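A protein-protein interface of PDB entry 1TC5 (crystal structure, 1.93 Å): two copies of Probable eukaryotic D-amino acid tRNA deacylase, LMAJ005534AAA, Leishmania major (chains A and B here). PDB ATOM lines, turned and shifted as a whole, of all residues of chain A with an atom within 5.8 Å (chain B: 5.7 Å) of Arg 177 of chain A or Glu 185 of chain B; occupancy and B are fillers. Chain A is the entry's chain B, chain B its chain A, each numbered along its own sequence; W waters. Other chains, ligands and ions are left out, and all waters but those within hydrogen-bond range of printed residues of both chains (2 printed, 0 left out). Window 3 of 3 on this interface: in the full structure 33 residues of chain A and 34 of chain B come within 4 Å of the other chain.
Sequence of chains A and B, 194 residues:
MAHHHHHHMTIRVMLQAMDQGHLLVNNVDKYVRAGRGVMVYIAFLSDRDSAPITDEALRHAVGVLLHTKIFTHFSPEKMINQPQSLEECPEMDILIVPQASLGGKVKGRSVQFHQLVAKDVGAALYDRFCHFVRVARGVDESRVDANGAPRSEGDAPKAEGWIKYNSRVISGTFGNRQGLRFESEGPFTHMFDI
Printed residues of chain B within 4 Å of Leu 180 of chain A: Glu 183, Ser 184 and Pro 187.
Printed residues of chain A within 4 Å of Glu 183 of chain B: Leu 180.
Printed residues of chain A within 4 Å of Ser 184 of chain B: Gly 179 and Leu 180.
Of the printed residues of chain A, Glu 185 of chain B touches Arg 177 (2.9 Å).
Printed residues of chain A within 4 Å of Gly 186 of chain B: Gln 178 (3.6 Å).
Of the printed residues of chain A, Pro 187 of chain B touches Gln 178 (3.2 Å) and Leu 180 (3.98 Å).
The nearest residue of chain B that does not touch Arg 177 of chain A is Gly 186 of chain B (4.4 Å).
The nearest printed residue of chain A that does not touch Glu 185 of chain B is Gly 179 of chain A (4.01 Å).
The backbone carbonyl oxygen of Ser 184 of chain B sits at hydrogen-bond distance from the backbone NH of Leu 180 of chain A (2.9 Å).
The guanidinium group (NH1) of Arg 177 of chain A is in salt-bridge range of the side-chain carboxylate (OE1) of Glu 185 of chain B, 3.7 Å away.
Water W2 lies within hydrogen-bond range of OE1 of Glu 185 of chain B (2.8 Å) and NH1 of Arg 177 of chain A (3.1 Å).
Water W1 lies within hydrogen-bond range of the backbone carbonyl oxygen of Leu 180 of chain A (2.9 Å) and the backbone carbonyl oxygen of Ser 184 of chain B (3.0 Å).
No position is printed for both chains.
Of the 7 pairs that touch across the chains among the printed residues, none has its exchanged pair printed and touching as well.
Among the printed residues, pairs that only touch across the chains: Gln 178 of chain A with Pro 187 of chain B, Leu 180 of chain A with Glu 183 of chain B, Gly 179 of chain A with Ser 184 of chain B, Gln 178 of chain A with Gly 186 of chain B and Leu 180 of chain A with Pro 187 of chain B.
Of the 12 printed residues of chain A, 4 touch a printed residue of chain B.
Hydrophobic or aromatic side chains of chain A within 4 Å of the printed part of chain B: Leu 180.
Of the 7 printed residues of chain B, 5 touch a printed residue of chain A.
Printed residues of chain B that touch a printed residue of chain A: Glu 183, Ser 184, Glu 185, Gly 186 and Pro 187.
Hydrophobic or aromatic side chains of chain B that line the printed part of chain A: Pro 187.
Among the printed residues, 7 pairs touch across the chains.
Among the printed residues, Asp or Glu carboxylates within 4 Å of a Lys or Arg side-chain nitrogen of the other chain: Arg 177 of chain A with Glu 185 of chain B (3.7 Å).
N of Asp 19 of chain B is in hydrogen-bond range of O of Glu 183 of chain B (2.9 Å).
The side-chain hydroxyl (OG) of Ser 184 of chain B lies within hydrogen-bond range of the backbone NH (N) of Gly 186 of chain B.
The backbone NH (N) of Leu 24 of chain A lies within hydrogen-bond range of the backbone carbonyl oxygen (O) of Gly 179 of chain A (2.8 Å).
The backbone NH (N) of Arg 177 of chain A sits at hydrogen-bond distance from the side-chain amide oxygen (OD1) of Asn 27 of chain A (2.9 Å).
The backbone carbonyl oxygen (O) of Thr 173 of chain A lies within hydrogen-bond range of the side-chain amide nitrogen (NE2) of Gln 178 of chain A, 2.9 Å away.
The side-chain amide nitrogen of Gln 178 of chain A is in hydrogen-bond range of the backbone carbonyl oxygen of Asn 176 of chain A, 2.8 Å away.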
ATOM      1  N   LEU A  24      15.365  22.630  10.953  1.00  0.00           N
ATOM      2  CA  LEU A  24      15.100  23.319   9.701  1.00  0.00           C
ATOM      3  C   LEU A  24      14.827  22.298   8.595  1.00  0.00           C
ATOM      4  O   LEU A  24      15.660  21.413   8.334  1.00  0.00           O
ATOM      5  CB  LEU A  24      16.304  24.196   9.352  1.00  0.00           C
ATOM      6  CG  LEU A  24      16.235  25.011   8.070  1.00  0.00           C
ATOM      7  CD1 LEU A  24      15.253  26.189   8.228  1.00  0.00           C
ATOM      8  CD2 LEU A  24      17.631  25.493   7.725  1.00  0.00           C
ATOM      9  N   VAL A  25      13.666  22.416   7.945  1.00  0.00           N
ATOM     10  CA  VAL A  25      13.231  21.417   6.964  1.00  0.00           C
ATOM     11  C   VAL A  25      13.161  21.900   5.502  1.00  0.00           C
ATOM     12  O   VAL A  25      12.999  21.075   4.620  1.00  0.00           O
ATOM     13  CB  VAL A  25      11.856  20.809   7.339  1.00  0.00           C
ATOM     14  CG1 VAL A  25      11.971  20.032   8.648  1.00  0.00           C
ATOM     15  CG2 VAL A  25      10.764  21.894   7.411  1.00  0.00           C
ATOM     16  N   ASN A  27      15.546  24.363   4.105  1.00  0.00           N
ATOM     17  CA  ASN A  27      16.818  25.040   3.796  1.00  0.00           C
ATOM     18  C   ASN A  27      16.799  26.562   4.009  1.00  0.00           C
ATOM     19  O   ASN A  27      17.802  27.233   3.752  1.00  0.00           O
ATOM     20  CB  ASN A  27      17.324  24.725   2.368  1.00  0.00           C
ATOM     21  CG  ASN A  27      18.054  23.416   2.289  1.00  0.00           C
ATOM     22  OD1 ASN A  27      18.563  22.905   3.285  1.00  0.00           O
ATOM     23  ND2 ASN A  27      18.106  22.861   1.109  1.00  0.00           N
ATOM     24  N   VAL A  28      15.684  27.097   4.503  1.00  0.00           N
ATOM     25  CA  VAL A  28      15.523  28.536   4.597  1.00  0.00           C
ATOM     26  C   VAL A  28      15.144  28.934   6.018  1.00  0.00           C
ATOM     27  O   VAL A  28      16.029  29.285   6.801  1.00  0.00           O
ATOM     28  CB  VAL A  28      14.534  29.054   3.540  1.00  0.00           C
ATOM     29  CG1 VAL A  28      14.325  30.585   3.667  1.00  0.00           C
ATOM     30  CG2 VAL A  28      15.047  28.699   2.139  1.00  0.00           C
ATOM     31  N   TYR A  31      11.056  25.750  10.577  1.00  0.00           N
ATOM     32  CA  TYR A  31      11.455  24.798  11.590  1.00  0.00           C
ATOM     33  C   TYR A  31      10.273  23.974  12.076  1.00  0.00           C
ATOM     34  O   TYR A  31       9.179  24.501  12.289  1.00  0.00           O
ATOM     35  CB  TYR A  31      12.066  25.530  12.768  1.00  0.00           C
ATOM     36  CG  TYR A  31      13.357  26.210  12.430  1.00  0.00           C
ATOM     37  CD1 TYR A  31      13.364  27.480  11.847  1.00  0.00           C
ATOM     38  CD2 TYR A  31      14.574  25.592  12.686  1.00  0.00           C
ATOM     39  CE1 TYR A  31      14.552  28.120  11.532  1.00  0.00           C
ATOM     40  CE2 TYR A  31      15.769  26.216  12.378  1.00  0.00           C
ATOM     41  CZ  TYR A  31      15.752  27.480  11.796  1.00  0.00           C
ATOM     42  OH  TYR A  31      16.928  28.103  11.490  1.00  0.00           O
ATOM     43  N   THR A 173      14.519  16.548   6.418  1.00  0.00           N
ATOM     44  CA  THR A 173      14.393  16.360   4.979  1.00  0.00           C
ATOM     45  C   THR A 173      15.718  15.839   4.499  1.00  0.00           C
ATOM     46  O   THR A 173      16.739  16.521   4.635  1.00  0.00           O
ATOM     47  CB  THR A 173      14.116  17.723   4.332  1.00  0.00           C
ATOM     48  OG1 THR A 173      12.909  18.276   4.871  1.00  0.00           O
ATOM     49  CG2 THR A 173      13.873  17.603   2.812  1.00  0.00           C
ATOM     50  N   GLY A 175      18.872  15.085   2.468  1.00  0.00           N
ATOM     51  CA  GLY A 175      19.623  15.853   1.500  1.00  0.00           C
ATOM     52  C   GLY A 175      19.614  17.342   1.768  1.00  0.00           C
ATOM     53  O   GLY A 175      20.307  18.076   1.083  1.00  0.00           O
ATOM     54  N   ASN A 176      18.835  17.801   2.751  1.00  0.00           N
ATOM     55  CA  ASN A 176      18.874  19.204   3.142  1.00  0.00           C
ATOM     56  C   ASN A 176      19.942  19.485   4.192  1.00  0.00           C
ATOM     57  O   ASN A 176      20.513  18.582   4.822  1.00  0.00           O
ATOM     58  CB  ASN A 176      17.517  19.708   3.669  1.00  0.00           C
ATOM     59  CG  ASN A 176      16.556  20.084   2.574  1.00  0.00           C
ATOM     60  OD1 ASN A 176      16.685  19.624   1.445  1.00  0.00           O
ATOM     61  ND2 ASN A 176      15.547  20.897   2.911  1.00  0.00           N
ATOM     62  N   ARG A 177      20.203  20.776   4.365  1.00  0.00           N
ATOM     63  CA  ARG A 177      21.015  21.287   5.458  1.00  0.00           C
ATOM     64  C   ARG A 177      20.188  21.276   6.749  1.00  0.00           C
ATOM     65  O   ARG A 177      19.105  21.862   6.821  1.00  0.00           O
ATOM     66  CB  ARG A 177      21.479  22.710   5.128  1.00  0.00           C
ATOM     67  CG  ARG A 177      22.352  23.362   6.166  1.00  0.00           C
ATOM     68  CD  ARG A 177      23.002  24.649   5.662  1.00  0.00           C
ATOM     69  NE  ARG A 177      21.977  25.630   5.275  1.00  0.00           N
ATOM     70  CZ  ARG A 177      21.227  26.345   6.114  1.00  0.00           C
ATOM     71  NH1 ARG A 177      21.391  26.257   7.432  1.00  0.00           N
ATOM     72  NH2 ARG A 177      20.313  27.174   5.631  1.00  0.00           N
ATOM     73  N   GLN A 178      20.743  20.647   7.771  1.00  0.00           N
ATOM     74  CA  GLN A 178      20.017  20.303   8.998  1.00  0.00           C
ATOM     75  C   GLN A 178      20.223  21.394  10.078  1.00  0.00           C
ATOM     76  O   GLN A 178      20.786  21.155  11.173  1.00  0.00           O
ATOM     77  CB  GLN A 178      20.488  18.918   9.474  1.00  0.00           C
ATOM     78  CG  GLN A 178      20.328  17.788   8.424  1.00  0.00           C
ATOM     79  CD  GLN A 178      18.882  17.587   7.924  1.00  0.00           C
ATOM     80  OE1 GLN A 178      17.934  17.570   8.712  1.00  0.00           O
ATOM     81  NE2 GLN A 178      18.725  17.421   6.616  1.00  0.00           N
ATOM     82  N   GLY A 179      19.753  22.605   9.758  1.00  0.00           N
ATOM     83  CA  GLY A 179      19.729  23.691  10.727  1.00  0.00           C
ATOM     84  C   GLY A 179      19.040  23.233  12.006  1.00  0.00           C
ATOM     85  O   GLY A 179      17.978  22.620  11.969  1.00  0.00           O
ATOM     86  N   LEU A 180      19.653  23.529  13.141  1.00  0.00           N
ATOM     87  CA  LEU A 180      19.243  22.942  14.412  1.00  0.00           C
ATOM     88  C   LEU A 180      19.300  23.927  15.564  1.00  0.00           C
ATOM     89  O   LEU A 180      20.268  24.657  15.695  1.00  0.00           O
ATOM     90  CB  LEU A 180      20.178  21.778  14.742  1.00  0.00           C
ATOM     91  CG  LEU A 180      19.855  20.994  16.009  1.00  0.00           C
ATOM     92  CD1 LEU A 180      18.485  20.313  15.889  1.00  0.00           C
ATOM     93  CD2 LEU A 180      20.935  19.971  16.275  1.00  0.00           C
ATOM     94  N   ALA B  17      29.530  21.135  13.986  1.00  0.00           N
ATOM     95  CA  ALA B  17      29.618  22.547  13.578  1.00  0.00           C
ATOM     96  C   ALA B  17      28.721  23.394  14.479  1.00  0.00           C
ATOM     97  O   ALA B  17      27.490  23.242  14.465  1.00  0.00           O
ATOM     98  CB  ALA B  17      29.191  22.719  12.131  1.00  0.00           C
ATOM     99  N   ASP B  19      27.377  27.130  15.807  1.00  0.00           N
ATOM    100  CA  ASP B  19      27.209  28.568  15.610  1.00  0.00           C
ATOM    101  C   ASP B  19      27.210  29.303  16.951  1.00  0.00           C
ATOM    102  O   ASP B  19      27.939  30.286  17.124  1.00  0.00           O
ATOM    103  CB  ASP B  19      25.902  28.894  14.890  1.00  0.00           C
ATOM    104  CG  ASP B  19      25.836  30.331  14.461  1.00  0.00           C
ATOM    105  OD1 ASP B  19      26.672  30.683  13.618  1.00  0.00           O
ATOM    106  OD2 ASP B  19      25.038  31.185  14.923  1.00  0.00           O
ATOM    107  N   GLU B 183      23.132  25.820  18.971  1.00  0.00           N
ATOM    108  CA  GLU B 183      22.590  26.280  17.683  1.00  0.00           C
ATOM    109  C   GLU B 183      23.621  25.997  16.599  1.00  0.00           C
ATOM    110  O   GLU B 183      24.814  26.276  16.765  1.00  0.00           O
ATOM    111  CB  GLU B 183      22.287  27.807  17.685  1.00  0.00           C
ATOM    112  CG  GLU B 183      21.219  28.260  18.674  1.00  0.00           C
ATOM    113  CD  GLU B 183      21.246  29.769  18.974  1.00  0.00           C
ATOM    114  OE1 GLU B 183      21.617  30.597  18.090  1.00  0.00           O
ATOM    115  OE2 GLU B 183      20.886  30.132  20.104  1.00  0.00           O
ATOM    116  N   SER B 184      23.135  25.503  15.465  1.00  0.00           N
ATOM    117  CA  SER B 184      23.980  25.127  14.362  1.00  0.00           C
ATOM    118  C   SER B 184      23.262  25.403  13.063  1.00  0.00           C
ATOM    119  O   SER B 184      22.064  25.191  12.959  1.00  0.00           O
ATOM    120  CB  SER B 184      24.344  23.651  14.503  1.00  0.00           C
ATOM    121  OG  SER B 184      24.999  23.146  13.369  1.00  0.00           O
ATOM    122  N   GLU B 185      24.023  25.841  12.058  1.00  0.00           N
ATOM    123  CA  GLU B 185      23.521  25.934  10.687  1.00  0.00           C
ATOM    124  C   GLU B 185      23.566  24.561   9.975  1.00  0.00           C
ATOM    125  O   GLU B 185      23.209  24.456   8.812  1.00  0.00           O
ATOM    126  CB  GLU B 185      24.359  26.953   9.897  1.00  0.00           C
ATOM    127  CG  GLU B 185      24.363  28.366  10.472  1.00  0.00           C
ATOM    128  CD  GLU B 185      23.006  29.040  10.333  1.00  0.00           C
ATOM    129  OE1 GLU B 185      22.575  29.260   9.185  1.00  0.00           O
ATOM    130  OE2 GLU B 185      22.354  29.323  11.365  1.00  0.00           O
ATOM    131  N   GLY B 186      24.000  23.505  10.665  1.00  0.00           N
ATOM    132  CA  GLY B 186      24.094  22.170  10.057  1.00  0.00           C
ATOM    133  C   GLY B 186      25.243  21.492  10.777  1.00  0.00           C
ATOM    134  O   GLY B 186      26.386  21.855  10.527  1.00  0.00           O
ATOM    135  N   PRO B 187      24.957  20.621  11.756  1.00  0.00           N
ATOM    136  CA  PRO B 187      26.014  20.044  12.588  1.00  0.00           C
ATOM    137  C   PRO B 187      27.100  19.286  11.831  1.00  0.00           C
ATOM    138  O   PRO B 187      28.224  19.307  12.323  1.00  0.00           O
ATOM    139  CB  PRO B 187      25.252  19.110  13.563  1.00  0.00           C
ATOM    140  CG  PRO B 187      23.841  19.633  13.579  1.00  0.00           C
ATOM    141  CD  PRO B 187      23.614  20.199  12.199  1.00  0.00           C
HETATM  142  O   HOH W   1      20.126  27.166  14.197  1.00  0.00           O
HETATM  143  O   HOH W   2      20.165  27.967   9.669  1.00  0.00           O
